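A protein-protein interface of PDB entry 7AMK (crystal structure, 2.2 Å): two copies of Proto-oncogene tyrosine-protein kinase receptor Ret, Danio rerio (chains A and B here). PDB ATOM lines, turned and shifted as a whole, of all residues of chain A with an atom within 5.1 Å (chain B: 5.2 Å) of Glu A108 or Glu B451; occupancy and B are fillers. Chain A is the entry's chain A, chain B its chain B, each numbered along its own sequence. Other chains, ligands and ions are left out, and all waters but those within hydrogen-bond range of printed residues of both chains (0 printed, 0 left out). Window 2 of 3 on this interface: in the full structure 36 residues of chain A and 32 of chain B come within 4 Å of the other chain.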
ATOM      1  N   ARG A   6      23.278  20.646  -0.531  1.00  0.00           N
ATOM      2  CA  ARG A   6      22.865  22.004  -0.902  1.00  0.00           C
ATOM      3  C   ARG A   6      21.448  22.091  -1.456  1.00  0.00           C
ATOM      4  O   ARG A   6      20.869  23.183  -1.467  1.00  0.00           O
ATOM      5  CB  ARG A   6      23.816  22.601  -1.957  1.00  0.00           C
ATOM      6  CG  ARG A   6      25.083  23.245  -1.402  1.00  0.00           C
ATOM      7  N   LEU A   7      20.879  20.982  -1.920  1.00  0.00           N
ATOM      8  CA  LEU A   7      19.600  21.003  -2.616  1.00  0.00           C
ATOM      9  C   LEU A   7      18.802  19.763  -2.244  1.00  0.00           C
ATOM     10  O   LEU A   7      19.326  18.649  -2.285  1.00  0.00           O
ATOM     11  CB  LEU A   7      19.822  21.072  -4.128  1.00  0.00           C
ATOM     12  CG  LEU A   7      18.616  20.882  -5.044  1.00  0.00           C
ATOM     13  CD1 LEU A   7      17.668  22.031  -4.873  1.00  0.00           C
ATOM     14  CD2 LEU A   7      19.067  20.780  -6.487  1.00  0.00           C
ATOM     15  N   TYR A   8      17.543  19.955  -1.873  1.00  0.00           N
ATOM     16  CA  TYR A   8      16.622  18.847  -1.677  1.00  0.00           C
ATOM     17  C   TYR A   8      15.575  18.903  -2.775  1.00  0.00           C
ATOM     18  O   TYR A   8      15.243  19.981  -3.278  1.00  0.00           O
ATOM     19  CB  TYR A   8      15.948  18.883  -0.306  1.00  0.00           C
ATOM     20  CG  TYR A   8      16.875  18.622   0.860  1.00  0.00           C
ATOM     21  CD1 TYR A   8      17.626  19.655   1.422  1.00  0.00           C
ATOM     22  CD2 TYR A   8      16.990  17.349   1.406  1.00  0.00           C
ATOM     23  CE1 TYR A   8      18.480  19.418   2.481  1.00  0.00           C
ATOM     24  CE2 TYR A   8      17.834  17.099   2.475  1.00  0.00           C
ATOM     25  CZ  TYR A   8      18.579  18.128   2.996  1.00  0.00           C
ATOM     26  OH  TYR A   8      19.416  17.882   4.045  1.00  0.00           O
ATOM     27  N   THR A  86      10.331  26.343  -5.289  1.00  0.00           N
ATOM     28  CA  THR A  86      11.604  26.457  -4.593  1.00  0.00           C
ATOM     29  C   THR A  86      11.372  27.097  -3.231  1.00  0.00           C
ATOM     30  O   THR A  86      10.969  28.258  -3.151  1.00  0.00           O
ATOM     31  CB  THR A  86      12.612  27.253  -5.416  1.00  0.00           C
ATOM     32  OG1 THR A  86      12.817  26.588  -6.665  1.00  0.00           O
ATOM     33  CG2 THR A  86      13.929  27.317  -4.692  1.00  0.00           C
ATOM     34  N   LEU A  87      11.606  26.326  -2.170  1.00  0.00           N
ATOM     35  CA  LEU A  87      11.547  26.779  -0.787  1.00  0.00           C
ATOM     36  C   LEU A  87      12.947  27.007  -0.240  1.00  0.00           C
ATOM     37  O   LEU A  87      13.906  26.344  -0.635  1.00  0.00           O
ATOM     38  CB  LEU A  87      10.847  25.749   0.105  1.00  0.00           C
ATOM     39  CG  LEU A  87       9.360  25.526  -0.117  1.00  0.00           C
ATOM     40  CD1 LEU A  87       8.902  24.291   0.645  1.00  0.00           C
ATOM     41  CD2 LEU A  87       8.599  26.767   0.314  1.00  0.00           C
ATOM     42  N   LYS A  88      13.047  27.929   0.701  1.00  0.00           N
ATOM     43  CA  LYS A  88      14.290  28.212   1.403  1.00  0.00           C
ATOM     44  C   LYS A  88      14.111  27.818   2.862  1.00  0.00           C
ATOM     45  O   LYS A  88      13.160  28.255   3.527  1.00  0.00           O
ATOM     46  CB  LYS A  88      14.677  29.693   1.276  1.00  0.00           C
ATOM     47  CG  LYS A  88      15.401  30.023  -0.024  1.00  0.00           C
ATOM     48  CD  LYS A  88      16.563  29.065  -0.233  1.00  0.00           C
ATOM     49  N   THR A 106      21.247  29.215   3.907  1.00  0.00           N
ATOM     50  CA  THR A 106      19.994  28.504   3.712  1.00  0.00           C
ATOM     51  C   THR A 106      20.199  27.282   2.821  1.00  0.00           C
ATOM     52  O   THR A 106      21.207  27.157   2.114  1.00  0.00           O
ATOM     53  CB  THR A 106      18.931  29.404   3.084  1.00  0.00           C
ATOM     54  OG1 THR A 106      19.394  29.821   1.801  1.00  0.00           O
ATOM     55  CG2 THR A 106      18.661  30.636   3.956  1.00  0.00           C
ATOM     56  N   VAL A 107      19.208  26.387   2.862  1.00  0.00           N
ATOM     57  CA  VAL A 107      19.105  25.230   1.978  1.00  0.00           C
ATOM     58  C   VAL A 107      17.972  25.475   0.992  1.00  0.00           C
ATOM     59  O   VAL A 107      16.948  26.068   1.344  1.00  0.00           O
ATOM     60  CB  VAL A 107      18.849  23.932   2.768  1.00  0.00           C
ATOM     61  CG1 VAL A 107      18.857  22.764   1.856  1.00  0.00           C
ATOM     62  CG2 VAL A 107      19.916  23.748   3.787  1.00  0.00           C
ATOM     63  N   GLU A 108      18.137  24.996  -0.229  1.00  0.00           N
ATOM     64  CA  GLU A 108      17.081  25.070  -1.222  1.00  0.00           C
ATOM     65  C   GLU A 108      16.318  23.742  -1.223  1.00  0.00           C
ATOM     66  O   GLU A 108      16.921  22.665  -1.310  1.00  0.00           O
ATOM     67  CB  GLU A 108      17.667  25.412  -2.598  1.00  0.00           C
ATOM     68  CG  GLU A 108      16.654  25.438  -3.751  1.00  0.00           C
ATOM     69  CD  GLU A 108      17.203  25.986  -5.082  1.00  0.00           C
ATOM     70  OE1 GLU A 108      18.206  26.753  -5.109  1.00  0.00           O
ATOM     71  OE2 GLU A 108      16.593  25.653  -6.125  1.00  0.00           O
ATOM     72  N   VAL A 109      14.999  23.816  -1.090  1.00  0.00           N
ATOM     73  CA  VAL A 109      14.134  22.649  -1.202  1.00  0.00           C
ATOM     74  C   VAL A 109      13.306  22.849  -2.460  1.00  0.00           C
ATOM     75  O   VAL A 109      12.398  23.691  -2.503  1.00  0.00           O
ATOM     76  CB  VAL A 109      13.248  22.456   0.034  1.00  0.00           C
ATOM     77  CG1 VAL A 109      12.451  21.190  -0.101  1.00  0.00           C
ATOM     78  CG2 VAL A 109      14.102  22.442   1.311  1.00  0.00           C
ATOM     79  N   LYS A 110      13.617  22.079  -3.491  1.00  0.00           N
ATOM     80  CA  LYS A 110      13.011  22.266  -4.800  1.00  0.00           C
ATOM     81  C   LYS A 110      11.950  21.185  -4.971  1.00  0.00           C
ATOM     82  O   LYS A 110      12.263  19.990  -5.022  1.00  0.00           O
ATOM     83  CB  LYS A 110      14.071  22.221  -5.900  1.00  0.00           C
ATOM     84  CG  LYS A 110      13.811  23.169  -7.050  1.00  0.00           C
ATOM     85  CD  LYS A 110      15.038  23.330  -7.946  1.00  0.00           C
ATOM     86  CE  LYS A 110      14.826  24.428  -8.980  1.00  0.00           C
ATOM     87  N   PRO B 447      15.045  32.746  -5.599  1.00  0.00           N
ATOM     88  CA  PRO B 447      15.567  31.587  -4.850  1.00  0.00           C
ATOM     89  C   PRO B 447      15.901  30.385  -5.722  1.00  0.00           C
ATOM     90  O   PRO B 447      16.862  29.663  -5.418  1.00  0.00           O
ATOM     91  CB  PRO B 447      14.432  31.273  -3.868  1.00  0.00           C
ATOM     92  CG  PRO B 447      13.748  32.588  -3.681  1.00  0.00           C
ATOM     93  CD  PRO B 447      13.784  33.252  -5.021  1.00  0.00           C
ATOM     94  N   GLU B 448      15.155  30.140  -6.803  1.00  0.00           N
ATOM     95  CA  GLU B 448      15.501  28.991  -7.636  1.00  0.00           C
ATOM     96  C   GLU B 448      16.834  29.173  -8.348  1.00  0.00           C
ATOM     97  O   GLU B 448      17.400  28.194  -8.839  1.00  0.00           O
ATOM     98  CB  GLU B 448      14.412  28.714  -8.675  1.00  0.00           C
ATOM     99  N   CYS B 449      17.348  30.395  -8.422  1.00  0.00           N
ATOM    100  CA  CYS B 449      18.572  30.663  -9.160  1.00  0.00           C
ATOM    101  C   CYS B 449      19.809  30.689  -8.269  1.00  0.00           C
ATOM    102  O   CYS B 449      20.864  31.143  -8.717  1.00  0.00           O
ATOM    103  CB  CYS B 449      18.459  31.994  -9.920  1.00  0.00           C
ATOM    104  SG  CYS B 449      17.227  32.087 -11.274  1.00  0.00           S
ATOM    105  N   GLN B 450      19.726  30.211  -7.027  1.00  0.00           N
ATOM    106  CA  GLN B 450      20.827  30.423  -6.093  1.00  0.00           C
ATOM    107  C   GLN B 450      21.668  29.175  -5.841  1.00  0.00           C
ATOM    108  O   GLN B 450      22.680  29.263  -5.143  1.00  0.00           O
ATOM    109  CB  GLN B 450      20.291  30.971  -4.757  1.00  0.00           C
ATOM    110  CG  GLN B 450      19.929  32.476  -4.792  1.00  0.00           C
ATOM    111  CD  GLN B 450      18.820  32.859  -3.830  1.00  0.00           C
ATOM    112  OE1 GLN B 450      18.679  32.288  -2.738  1.00  0.00           O
ATOM    113  NE2 GLN B 450      18.017  33.843  -4.231  1.00  0.00           N
ATOM    114  N   GLU B 451      21.267  28.026  -6.368  1.00  0.00           N
ATOM    115  CA  GLU B 451      22.084  26.820  -6.360  1.00  0.00           C
ATOM    116  C   GLU B 451      22.147  26.327  -7.796  1.00  0.00           C
ATOM    117  O   GLU B 451      21.142  25.853  -8.335  1.00  0.00           O
ATOM    118  CB  GLU B 451      21.498  25.759  -5.439  1.00  0.00           C
ATOM    119  CG  GLU B 451      21.652  26.064  -3.960  1.00  0.00           C
ATOM    120  CD  GLU B 451      23.102  25.999  -3.475  1.00  0.00           C
ATOM    121  OE1 GLU B 451      23.985  25.597  -4.249  1.00  0.00           O
ATOM    122  OE2 GLU B 451      23.354  26.348  -2.304  1.00  0.00           O
ATOM    123  N   LEU B 452      23.314  26.461  -8.414  1.00  0.00           N
ATOM    124  CA  LEU B 452      23.545  26.136  -9.811  1.00  0.00           C
ATOM    125  C   LEU B 452      24.502  24.951  -9.929  1.00  0.00           C
ATOM    126  O   LEU B 452      25.422  24.781  -9.118  1.00  0.00           O
ATOM    127  CB  LEU B 452      24.129  27.337 -10.557  1.00  0.00           C
ATOM    128  CG  LEU B 452      23.392  28.671 -10.515  1.00  0.00           C
ATOM    129  CD1 LEU B 452      24.251  29.739 -11.181  1.00  0.00           C
ATOM    130  CD2 LEU B 452      22.054  28.563 -11.223  1.00  0.00           C
ATOM    131  N   GLU B 453      24.288  24.133 -10.952  1.00  0.00           N
ATOM    132  CA  GLU B 453      25.081  22.929 -11.142  1.00  0.00           C
ATOM    133  C   GLU B 453      25.510  22.849 -12.599  1.00  0.00           C
ATOM    134  O   GLU B 453      24.679  22.921 -13.505  1.00  0.00           O
ATOM    135  CB  GLU B 453      24.310  21.673 -10.709  1.00  0.00           C
ATOM    136  CG  GLU B 453      25.232  20.416 -10.597  1.00  0.00           C
ATOM    137  CD  GLU B 453      24.688  19.346  -9.645  1.00  0.00           C
ATOM    138  OE1 GLU B 453      23.671  19.603  -8.955  1.00  0.00           O
ATOM    139  OE2 GLU B 453      25.283  18.243  -9.580  1.00  0.00           O
ATOM    140  N   VAL B 473      27.837  26.172  -7.897  1.00  0.00           N
ATOM    141  CA  VAL B 473      27.946  27.541  -7.401  1.00  0.00           C
ATOM    142  C   VAL B 473      26.751  27.816  -6.498  1.00  0.00           C
ATOM    143  O   VAL B 473      25.597  27.593  -6.883  1.00  0.00           O
ATOM    144  CB  VAL B 473      28.013  28.568  -8.545  1.00  0.00           C
ATOM    145  CG1 VAL B 473      28.184  29.972  -7.968  1.00  0.00           C
ATOM    146  CG2 VAL B 473      29.161  28.233  -9.489  1.00  0.00           C
ATOM    147  N   SER B 474      27.032  28.295  -5.305  1.00  0.00           N
ATOM    148  CA  SER B 474      26.020  28.558  -4.300  1.00  0.00           C
ATOM    149  C   SER B 474      26.042  30.051  -3.979  1.00  0.00           C
ATOM    150  O   SER B 474      27.096  30.610  -3.660  1.00  0.00           O
ATOM    151  CB  SER B 474      26.287  27.678  -3.067  1.00  0.00           C
ATOM    152  OG  SER B 474      25.361  27.940  -2.024  1.00  0.00           O
ATOM    153  N   PHE B 475      24.889  30.693  -4.084  1.00  0.00           N
ATOM    154  CA  PHE B 475      24.727  32.113  -3.788  1.00  0.00           C
ATOM    155  C   PHE B 475      24.047  32.245  -2.429  1.00  0.00           C
ATOM    156  O   PHE B 475      22.848  31.994  -2.295  1.00  0.00           O
ATOM    157  CB  PHE B 475      23.920  32.795  -4.884  1.00  0.00           C
ATOM    158  CG  PHE B 475      24.681  32.999  -6.137  1.00  0.00           C
ATOM    159  CD1 PHE B 475      25.587  34.038  -6.235  1.00  0.00           C
ATOM    160  CD2 PHE B 475      24.523  32.144  -7.211  1.00  0.00           C
ATOM    161  CE1 PHE B 475      26.323  34.232  -7.376  1.00  0.00           C
ATOM    162  CE2 PHE B 475      25.254  32.330  -8.365  1.00  0.00           C
ATOM    163  CZ  PHE B 475      26.152  33.375  -8.455  1.00  0.00           C
ATOM    164  N   GLN B 476      24.805  32.656  -1.421  1.00  0.00           N
ATOM    165  CA  GLN B 476      24.281  32.680  -0.062  1.00  0.00           C
ATOM    166  C   GLN B 476      24.074  34.112   0.419  1.00  0.00           C
ATOM    167  O   GLN B 476      24.479  35.052  -0.261  1.00  0.00           O
ATOM    168  CB  GLN B 476      25.219  31.910   0.883  1.00  0.00           C
ATOM    169  CG  GLN B 476      25.220  30.382   0.688  1.00  0.00           C
ATOM    170  CD  GLN B 476      23.918  29.691   1.155  1.00  0.00           C
ATOM    171  OE1 GLN B 476      22.964  30.344   1.574  1.00  0.00           O
ATOM    172  NE2 GLN B 476      23.890  28.362   1.072  1.00  0.00           N
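The backbone NH of Thr A106 lies within hydrogen-bond range of the side-chain amide oxygen of Gln B476 (3.1 Å).
The side-chain carboxylate (OE1) of Glu A108 lies close to the backbone carbonyl oxygen (O) of Pro B447, at 3.2 Å.
Glu A108 touches just these residues of chain B: Pro B447 (3.2 Å), Glu B448 (3.8 Å) and Glu B451 (3.5 Å).
Of the printed residues of chain A, Glu B451 touches Arg A6 (3.7 Å) and Glu A108 (3.5 Å).
Of the printed residues of chain B, Arg A6 touches Glu B451 (3.7 Å).
Printed residues of chain A within 4 Å of Glu B448: Thr A86 and Glu A108.
Of the printed residues of chain B, Thr A106 touches Gln B476.
Of the printed residues of chain B, Thr A86 touches Pro B447 and Glu B448.
Printed residues of chain A within 4 Å of Pro B447: Thr A86 (3.8 Å) and Glu A108 (3.2 Å).
Gln B450 touches none of the printed residues of chain A.
The nearest residue of chain B that does not touch Glu A108 is Gln B450 (4.2 Å).
The nearest printed residue of chain A that does not touch Glu B451 is Thr A106 (5.0 Å).
Among the printed residues, merely in contact across the chains: Thr A86 with Glu B448 (3.3 Å), Glu A108 with Glu B451 (3.5 Å), Arg A6 with Glu B451 (3.7 Å), Thr A86 with Pro B447 (3.8 Å) and Glu A108 with Glu B448 (3.8 Å).
The backbone NH (N) of Tyr A8 lies within hydrogen-bond range of the backbone carbonyl oxygen (O) of Glu A108, 2.8 Å away.
The side-chain carboxylate of Glu B451 lies within hydrogen-bond range of the side-chain hydroxyl of Ser B474 (2.6 Å).
The side-chain amide nitrogen (NE2) of Gln B476 sits at hydrogen-bond distance from the side-chain hydroxyl (OG) of Ser B474.
Of the 11 printed residues of chain A, 4 touch a printed residue of chain B.
Printed residues of chain A that touch a printed residue of chain B: Arg A6, Thr A86, Thr A106 and Glu A108.
Printed residues of chain B that touch a printed residue of chain A: Pro B447, Glu B448, Glu B451 and Gln B476.
Among the printed residues, 7 pairs touch across the chains.
No position is printed for both chains.
Of the 7 pairs that touch across the chains among the printed residues, none has its exchanged pair printed and touching as well.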
